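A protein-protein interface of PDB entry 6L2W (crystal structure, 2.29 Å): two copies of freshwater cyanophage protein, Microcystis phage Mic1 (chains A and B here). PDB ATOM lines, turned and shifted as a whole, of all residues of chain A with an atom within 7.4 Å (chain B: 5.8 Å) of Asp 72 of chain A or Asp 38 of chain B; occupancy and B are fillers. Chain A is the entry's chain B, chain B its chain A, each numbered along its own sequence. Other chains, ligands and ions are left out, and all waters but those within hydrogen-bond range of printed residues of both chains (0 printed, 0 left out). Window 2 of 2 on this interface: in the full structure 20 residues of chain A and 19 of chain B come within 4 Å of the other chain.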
ATOM      1  N   ASN A  67      18.327   4.630 -15.603  1.00  0.00           N
ATOM      2  CA  ASN A  67      18.356   4.483 -17.048  1.00  0.00           C
ATOM      3  C   ASN A  67      18.919   5.737 -17.736  1.00  0.00           C
ATOM      4  O   ASN A  67      19.107   5.700 -18.936  1.00  0.00           O
ATOM      5  CB  ASN A  67      16.993   4.074 -17.631  1.00  0.00           C
ATOM      6  CG  ASN A  67      15.874   5.080 -17.470  1.00  0.00           C
ATOM      7  OD1 ASN A  67      16.091   6.275 -17.267  1.00  0.00           O
ATOM      8  ND2 ASN A  67      14.653   4.595 -17.593  1.00  0.00           N
ATOM      9  N   SER A  69      17.569   8.502 -18.441  1.00  0.00           N
ATOM     10  CA  SER A  69      16.549   9.282 -19.147  1.00  0.00           C
ATOM     11  C   SER A  69      16.219  10.569 -18.370  1.00  0.00           C
ATOM     12  O   SER A  69      16.033  10.581 -17.141  1.00  0.00           O
ATOM     13  CB  SER A  69      15.310   8.451 -19.375  1.00  0.00           C
ATOM     14  OG  SER A  69      14.349   9.133 -20.176  1.00  0.00           O
ATOM     15  N   LEU A  70      16.138  11.659 -19.112  1.00  0.00           N
ATOM     16  CA  LEU A  70      15.608  12.891 -18.579  1.00  0.00           C
ATOM     17  C   LEU A  70      14.150  13.027 -19.030  1.00  0.00           C
ATOM     18  O   LEU A  70      13.442  13.943 -18.603  1.00  0.00           O
ATOM     19  CB  LEU A  70      16.484  14.045 -19.073  1.00  0.00           C
ATOM     20  CG  LEU A  70      17.916  14.001 -18.546  1.00  0.00           C
ATOM     21  CD1 LEU A  70      18.856  14.807 -19.429  1.00  0.00           C
ATOM     22  CD2 LEU A  70      17.963  14.485 -17.106  1.00  0.00           C
ATOM     23  N   GLY A  71      13.744  12.089 -19.863  1.00  0.00           N
ATOM     24  CA  GLY A  71      12.412  12.138 -20.481  1.00  0.00           C
ATOM     25  C   GLY A  71      11.498  11.003 -20.100  1.00  0.00           C
ATOM     26  O   GLY A  71      11.347  10.757 -18.920  1.00  0.00           O
ATOM     27  N   ASP A  72      10.919  10.348 -21.083  1.00  0.00           N
ATOM     28  CA  ASP A  72       9.891   9.311 -20.831  1.00  0.00           C
ATOM     29  C   ASP A  72      10.352   7.906 -21.207  1.00  0.00           C
ATOM     30  O   ASP A  72       9.505   7.157 -21.652  1.00  0.00           O
ATOM     31  CB  ASP A  72       8.582   9.657 -21.538  1.00  0.00           C
ATOM     32  CG  ASP A  72       8.633   9.630 -23.055  1.00  0.00           C
ATOM     33  OD1 ASP A  72       9.713   9.432 -23.603  1.00  0.00           O
ATOM     34  OD2 ASP A  72       7.584   9.819 -23.666  1.00  0.00           O
ATOM     35  N   PHE A  73      11.617   7.567 -21.062  1.00  0.00           N
ATOM     36  CA  PHE A  73      12.057   6.175 -21.314  1.00  0.00           C
ATOM     37  C   PHE A  73      11.671   5.403 -20.057  1.00  0.00           C
ATOM     38  O   PHE A  73      12.165   5.749 -19.008  1.00  0.00           O
ATOM     39  CB  PHE A  73      13.540   6.134 -21.673  1.00  0.00           C
ATOM     40  CG  PHE A  73      14.070   4.795 -22.107  1.00  0.00           C
ATOM     41  CD1 PHE A  73      13.853   4.323 -23.384  1.00  0.00           C
ATOM     42  CD2 PHE A  73      14.819   4.020 -21.247  1.00  0.00           C
ATOM     43  CE1 PHE A  73      14.358   3.102 -23.787  1.00  0.00           C
ATOM     44  CE2 PHE A  73      15.319   2.797 -21.652  1.00  0.00           C
ATOM     45  CZ  PHE A  73      15.086   2.338 -22.918  1.00  0.00           C
ATOM     46  N   ARG A  74      10.810   4.419 -20.188  1.00  0.00           N
ATOM     47  CA  ARG A  74      10.224   3.708 -19.031  1.00  0.00           C
ATOM     48  C   ARG A  74      10.792   2.304 -18.867  1.00  0.00           C
ATOM     49  O   ARG A  74      10.056   1.435 -18.445  1.00  0.00           O
ATOM     50  CB  ARG A  74       8.712   3.648 -19.228  1.00  0.00           C
ATOM     51  CG  ARG A  74       8.282   2.945 -20.503  1.00  0.00           C
ATOM     52  CD  ARG A  74       6.806   3.126 -20.717  1.00  0.00           C
ATOM     53  NE  ARG A  74       6.309   2.422 -21.873  1.00  0.00           N
ATOM     54  CZ  ARG A  74       5.897   1.178 -21.857  1.00  0.00           C
ATOM     55  NH1 ARG A  74       5.713   0.549 -20.720  1.00  0.00           N
ATOM     56  NH2 ARG A  74       5.667   0.549 -22.985  1.00  0.00           N
ATOM     57  N   TYR A  75      12.052   2.124 -19.144  1.00  0.00           N
ATOM     58  CA  TYR A  75      12.682   0.826 -19.008  1.00  0.00           C
ATOM     59  C   TYR A  75      14.000   0.971 -18.253  1.00  0.00           C
ATOM     60  O   TYR A  75      14.741   1.907 -18.464  1.00  0.00           O
ATOM     61  CB  TYR A  75      12.966   0.201 -20.380  1.00  0.00           C
ATOM     62  CG  TYR A  75      11.780   0.170 -21.309  1.00  0.00           C
ATOM     63  CD1 TYR A  75      11.493   1.230 -22.145  1.00  0.00           C
ATOM     64  CD2 TYR A  75      10.911  -0.897 -21.314  1.00  0.00           C
ATOM     65  CE1 TYR A  75      10.399   1.209 -22.998  1.00  0.00           C
ATOM     66  CE2 TYR A  75       9.815  -0.939 -22.159  1.00  0.00           C
ATOM     67  CZ  TYR A  75       9.557   0.115 -23.015  1.00  0.00           C
ATOM     68  OH  TYR A  75       8.457   0.081 -23.836  1.00  0.00           O
ATOM     69  N   LEU A  87       7.847   0.339 -16.655  1.00  0.00           N
ATOM     70  CA  LEU A  87       6.756   1.062 -16.014  1.00  0.00           C
ATOM     71  C   LEU A  87       5.690   1.365 -17.077  1.00  0.00           C
ATOM     72  O   LEU A  87       6.075   1.766 -18.175  1.00  0.00           O
ATOM     73  CB  LEU A  87       7.332   2.350 -15.419  1.00  0.00           C
ATOM     74  CG  LEU A  87       6.323   3.421 -15.045  1.00  0.00           C
ATOM     75  CD1 LEU A  87       5.669   3.112 -13.714  1.00  0.00           C
ATOM     76  CD2 LEU A  87       6.997   4.769 -14.996  1.00  0.00           C
ATOM     77  N   ASN A  94       1.511  11.249 -17.825  1.00  0.00           N
ATOM     78  CA  ASN A  94       2.906  11.650 -18.090  1.00  0.00           C
ATOM     79  C   ASN A  94       3.854  11.034 -17.044  1.00  0.00           C
ATOM     80  O   ASN A  94       3.978  11.528 -15.925  1.00  0.00           O
ATOM     81  CB  ASN A  94       3.068  13.171 -18.116  1.00  0.00           C
ATOM     82  CG  ASN A  94       4.491  13.590 -18.427  1.00  0.00           C
ATOM     83  OD1 ASN A  94       5.432  13.106 -17.808  1.00  0.00           O
ATOM     84  ND2 ASN A  94       4.660  14.489 -19.382  1.00  0.00           N
ATOM     85  N   LEU A  95       4.586  10.000 -17.445  1.00  0.00           N
ATOM     86  CA  LEU A  95       5.384   9.170 -16.526  1.00  0.00           C
ATOM     87  C   LEU A  95       6.722   9.832 -16.171  1.00  0.00           C
ATOM     88  O   LEU A  95       7.489   9.273 -15.398  1.00  0.00           O
ATOM     89  CB  LEU A  95       5.622   7.812 -17.192  1.00  0.00           C
ATOM     90  CG  LEU A  95       4.354   7.029 -17.521  1.00  0.00           C
ATOM     91  CD1 LEU A  95       4.671   5.754 -18.277  1.00  0.00           C
ATOM     92  CD2 LEU A  95       3.589   6.720 -16.252  1.00  0.00           C
ATOM     93  N   GLU A  96       7.025  10.995 -16.724  1.00  0.00           N
ATOM     94  CA  GLU A  96       8.327  11.617 -16.502  1.00  0.00           C
ATOM     95  C   GLU A  96       8.626  11.701 -14.995  1.00  0.00           C
ATOM     96  O   GLU A  96       9.776  11.488 -14.586  1.00  0.00           O
ATOM     97  CB  GLU A  96       8.395  13.001 -17.164  1.00  0.00           C
ATOM     98  CG  GLU A  96       8.785  12.957 -18.638  1.00  0.00           C
ATOM     99  CD  GLU A  96       7.797  13.542 -19.642  1.00  0.00           C
ATOM    100  OE1 GLU A  96       7.133  12.752 -20.367  1.00  0.00           O
ATOM    101  OE2 GLU A  96       7.708  14.786 -19.720  1.00  0.00           O
ATOM    102  N   ILE A  99       9.358   8.310 -13.482  1.00  0.00           N
ATOM    103  CA  ILE A  99      10.620   7.812 -14.011  1.00  0.00           C
ATOM    104  C   ILE A  99      11.759   8.465 -13.232  1.00  0.00           C
ATOM    105  O   ILE A  99      12.687   7.776 -12.842  1.00  0.00           O
ATOM    106  CB  ILE A  99      10.721   8.037 -15.533  1.00  0.00           C
ATOM    107  CG1 ILE A  99       9.786   7.082 -16.276  1.00  0.00           C
ATOM    108  CG2 ILE A  99      12.151   7.897 -16.036  1.00  0.00           C
ATOM    109  CD1 ILE A  99       9.460   7.518 -17.684  1.00  0.00           C
ATOM    110  N   ILE B  36      15.383  11.566 -28.375  1.00  0.00           N
ATOM    111  CA  ILE B  36      14.004  11.148 -28.715  1.00  0.00           C
ATOM    112  C   ILE B  36      13.016  11.746 -27.703  1.00  0.00           C
ATOM    113  O   ILE B  36      13.129  11.512 -26.500  1.00  0.00           O
ATOM    114  CB  ILE B  36      13.877   9.610 -28.793  1.00  0.00           C
ATOM    115  CG1 ILE B  36      14.789   9.002 -29.861  1.00  0.00           C
ATOM    116  CG2 ILE B  36      12.428   9.199 -29.008  1.00  0.00           C
ATOM    117  CD1 ILE B  36      14.913   7.509 -29.761  1.00  0.00           C
ATOM    118  N   GLU B  37      12.006  12.446 -28.217  1.00  0.00           N
ATOM    119  CA  GLU B  37      11.042  13.146 -27.377  1.00  0.00           C
ATOM    120  C   GLU B  37      10.004  12.145 -26.858  1.00  0.00           C
ATOM    121  O   GLU B  37       9.853  11.936 -25.647  1.00  0.00           O
ATOM    122  CB  GLU B  37      10.362  14.265 -28.170  1.00  0.00           C
ATOM    123  CG  GLU B  37      11.332  15.289 -28.744  1.00  0.00           C
ATOM    124  CD  GLU B  37      10.865  16.027 -29.991  1.00  0.00           C
ATOM    125  OE1 GLU B  37       9.713  15.799 -30.430  1.00  0.00           O
ATOM    126  OE2 GLU B  37      11.657  16.834 -30.524  1.00  0.00           O
ATOM    127  N   ASP B  38       9.288  11.534 -27.789  1.00  0.00           N
ATOM    128  CA  ASP B  38       8.137  10.714 -27.438  1.00  0.00           C
ATOM    129  C   ASP B  38       8.513   9.258 -27.728  1.00  0.00           C
ATOM    130  O   ASP B  38       8.089   8.705 -28.743  1.00  0.00           O
ATOM    131  CB  ASP B  38       6.901  11.219 -28.190  1.00  0.00           C
ATOM    132  CG  ASP B  38       5.649  10.386 -28.004  1.00  0.00           C
ATOM    133  OD1 ASP B  38       5.603   9.632 -27.023  1.00  0.00           O
ATOM    134  OD2 ASP B  38       4.729  10.500 -28.850  1.00  0.00           O
ATOM    135  N   TYR B  39       9.317   8.666 -26.829  1.00  0.00           N
ATOM    136  CA  TYR B  39      10.054   7.439 -27.152  1.00  0.00           C
ATOM    137  C   TYR B  39       9.089   6.336 -27.605  1.00  0.00           C
ATOM    138  O   TYR B  39       9.395   5.565 -28.492  1.00  0.00           O
ATOM    139  CB  TYR B  39      10.915   6.952 -25.980  1.00  0.00           C
ATOM    140  CG  TYR B  39      11.653   5.677 -26.295  1.00  0.00           C
ATOM    141  CD1 TYR B  39      12.927   5.708 -26.828  1.00  0.00           C
ATOM    142  CD2 TYR B  39      11.047   4.440 -26.151  1.00  0.00           C
ATOM    143  CE1 TYR B  39      13.603   4.540 -27.164  1.00  0.00           C
ATOM    144  CE2 TYR B  39      11.699   3.266 -26.503  1.00  0.00           C
ATOM    145  CZ  TYR B  39      12.986   3.313 -27.018  1.00  0.00           C
ATOM    146  OH  TYR B  39      13.643   2.166 -27.370  1.00  0.00           O
ATOM    147  N   ASP B  40       7.919   6.285 -27.009  1.00  0.00           N
ATOM    148  CA  ASP B  40       7.040   5.167 -27.237  1.00  0.00           C
ATOM    149  C   ASP B  40       6.457   5.240 -28.646  1.00  0.00           C
ATOM    150  O   ASP B  40       6.027   4.240 -29.164  1.00  0.00           O
ATOM    151  CB  ASP B  40       5.984   5.068 -26.136  1.00  0.00           C
ATOM    152  CG  ASP B  40       6.551   4.411 -24.886  1.00  0.00           C
ATOM    153  OD1 ASP B  40       7.412   3.501 -25.029  1.00  0.00           O
ATOM    154  OD2 ASP B  40       6.146   4.811 -23.782  1.00  0.00           O
ATOM    155  N   ASN B  41       6.461   6.405 -29.269  1.00  0.00           N
ATOM    156  CA  ASN B  41       5.842   6.526 -30.574  1.00  0.00           C
ATOM    157  C   ASN B  41       6.938   6.624 -31.632  1.00  0.00           C
ATOM    158  O   ASN B  41       6.641   6.859 -32.792  1.00  0.00           O
ATOM    159  CB  ASN B  41       4.847   7.689 -30.612  1.00  0.00           C
ATOM    160  CG  ASN B  41       3.650   7.418 -29.726  1.00  0.00           C
ATOM    161  OD1 ASN B  41       2.903   6.466 -29.945  1.00  0.00           O
ATOM    162  ND2 ASN B  41       3.467   8.237 -28.707  1.00  0.00           N
ATOM    163  N   PHE B  42       8.185   6.390 -31.243  1.00  0.00           N
ATOM    164  CA  PHE B  42       9.279   6.680 -32.119  1.00  0.00           C
ATOM    165  C   PHE B  42       9.826   5.413 -32.791  1.00  0.00           C
ATOM    166  O   PHE B  42      10.032   4.415 -32.149  1.00  0.00           O
ATOM    167  CB  PHE B  42      10.412   7.349 -31.348  1.00  0.00           C
ATOM    168  CG  PHE B  42      11.544   7.712 -32.258  1.00  0.00           C
ATOM    169  CD1 PHE B  42      11.478   8.863 -33.025  1.00  0.00           C
ATOM    170  CD2 PHE B  42      12.621   6.863 -32.414  1.00  0.00           C
ATOM    171  CE1 PHE B  42      12.505   9.184 -33.895  1.00  0.00           C
ATOM    172  CE2 PHE B  42      13.645   7.182 -33.290  1.00  0.00           C
ATOM    173  CZ  PHE B  42      13.583   8.339 -34.032  1.00  0.00           C
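The backbone NH (N) of Tyr 39 of chain B is in hydrogen-bond range of the side-chain carboxylate (OD1) of Asp 72 of chain A, at 3.3 Å. OD2 of Asp 40 of chain B is in salt-bridge range of NE of Arg 74 of chain A, 3.1 Å away. The side-chain carboxylate (OD1) of Asp 72 of chain A sits close to the backbone carbonyl oxygen (O) of Glu 37 of chain B, 3.2 Å away.
The side-chain amide nitrogen (ND2) of Asn 41 of chain B lies within hydrogen-bond range of the side-chain carboxylate (OD2) of Asp 38 of chain B (2.6 Å). The backbone carbonyl oxygen (O) of Phe 73 of chain A is in hydrogen-bond range of the side-chain amide nitrogen (ND2) of Asn 67 of chain A (3.1 Å). ND2 of Asn 67 of chain A is in hydrogen-bond range of O of Tyr 75 of chain A, at 2.8 Å. The backbone NH of Phe 73 of chain A sits at hydrogen-bond distance from the side-chain hydroxyl of Ser 69 of chain A. The guanidinium group (NH2) of Arg 74 of chain A lies within hydrogen-bond range of the side-chain hydroxyl (OH) of Tyr 75 of chain A, 3.0 Å away. The guanidinium group of Arg 74 of chain A lies within hydrogen-bond range of the backbone carbonyl oxygen of Leu 87 of chain A, at 2.8 Å.
Asp 72 of chain A touches Asp 38 of chain B (OD2 to OD1, 3.9 Å). Tyr 39 of chain B touches Phe 73 of chain A (CZ to CE1, 3.5 Å). OD1 of Asp 40 of chain B touches OH of Tyr 75 of chain A (3.8 Å).
Of chain B, only Glu 37 (3.2 Å), Asp 38 (3.9 Å) and Tyr 39 (3.3 Å) come within 4 Å of Asp 72 of chain A. Of chain A, only Asp 72 comes within 4 Å of Asp 38 of chain B. Of the printed residues of chain A, Glu 37 of chain B touches Asp 72 (3.2 Å). Of the printed residues of chain B, Arg 74 of chain A touches Asp 40 (3.1 Å). Of the printed residues of chain A, Tyr 39 of chain B touches Asp 72 and Phe 73. Glu 96 of chain A touches none of the printed residues of chain B. Gly 71 of chain A touches none of the printed residues of chain B. The nearest printed residue of chain B that does not touch Arg 74 of chain A is Tyr 39 of chain B (6.0 Å).
Printed residues of chain A that touch a printed residue of chain B: Asp 72, Phe 73, Arg 74 and Tyr 75. Hydrophobic or aromatic side chains of chain A within 4 Å of the printed part of chain B: Phe 73 and Tyr 75. Of the 7 printed residues of chain B, 4 touch a printed residue of chain A. Hydrophobic or aromatic side chains of chain B that line the printed part of chain A: Tyr 39. Among the printed residues, 6 pairs touch across the chains.
No position is printed for both chains.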
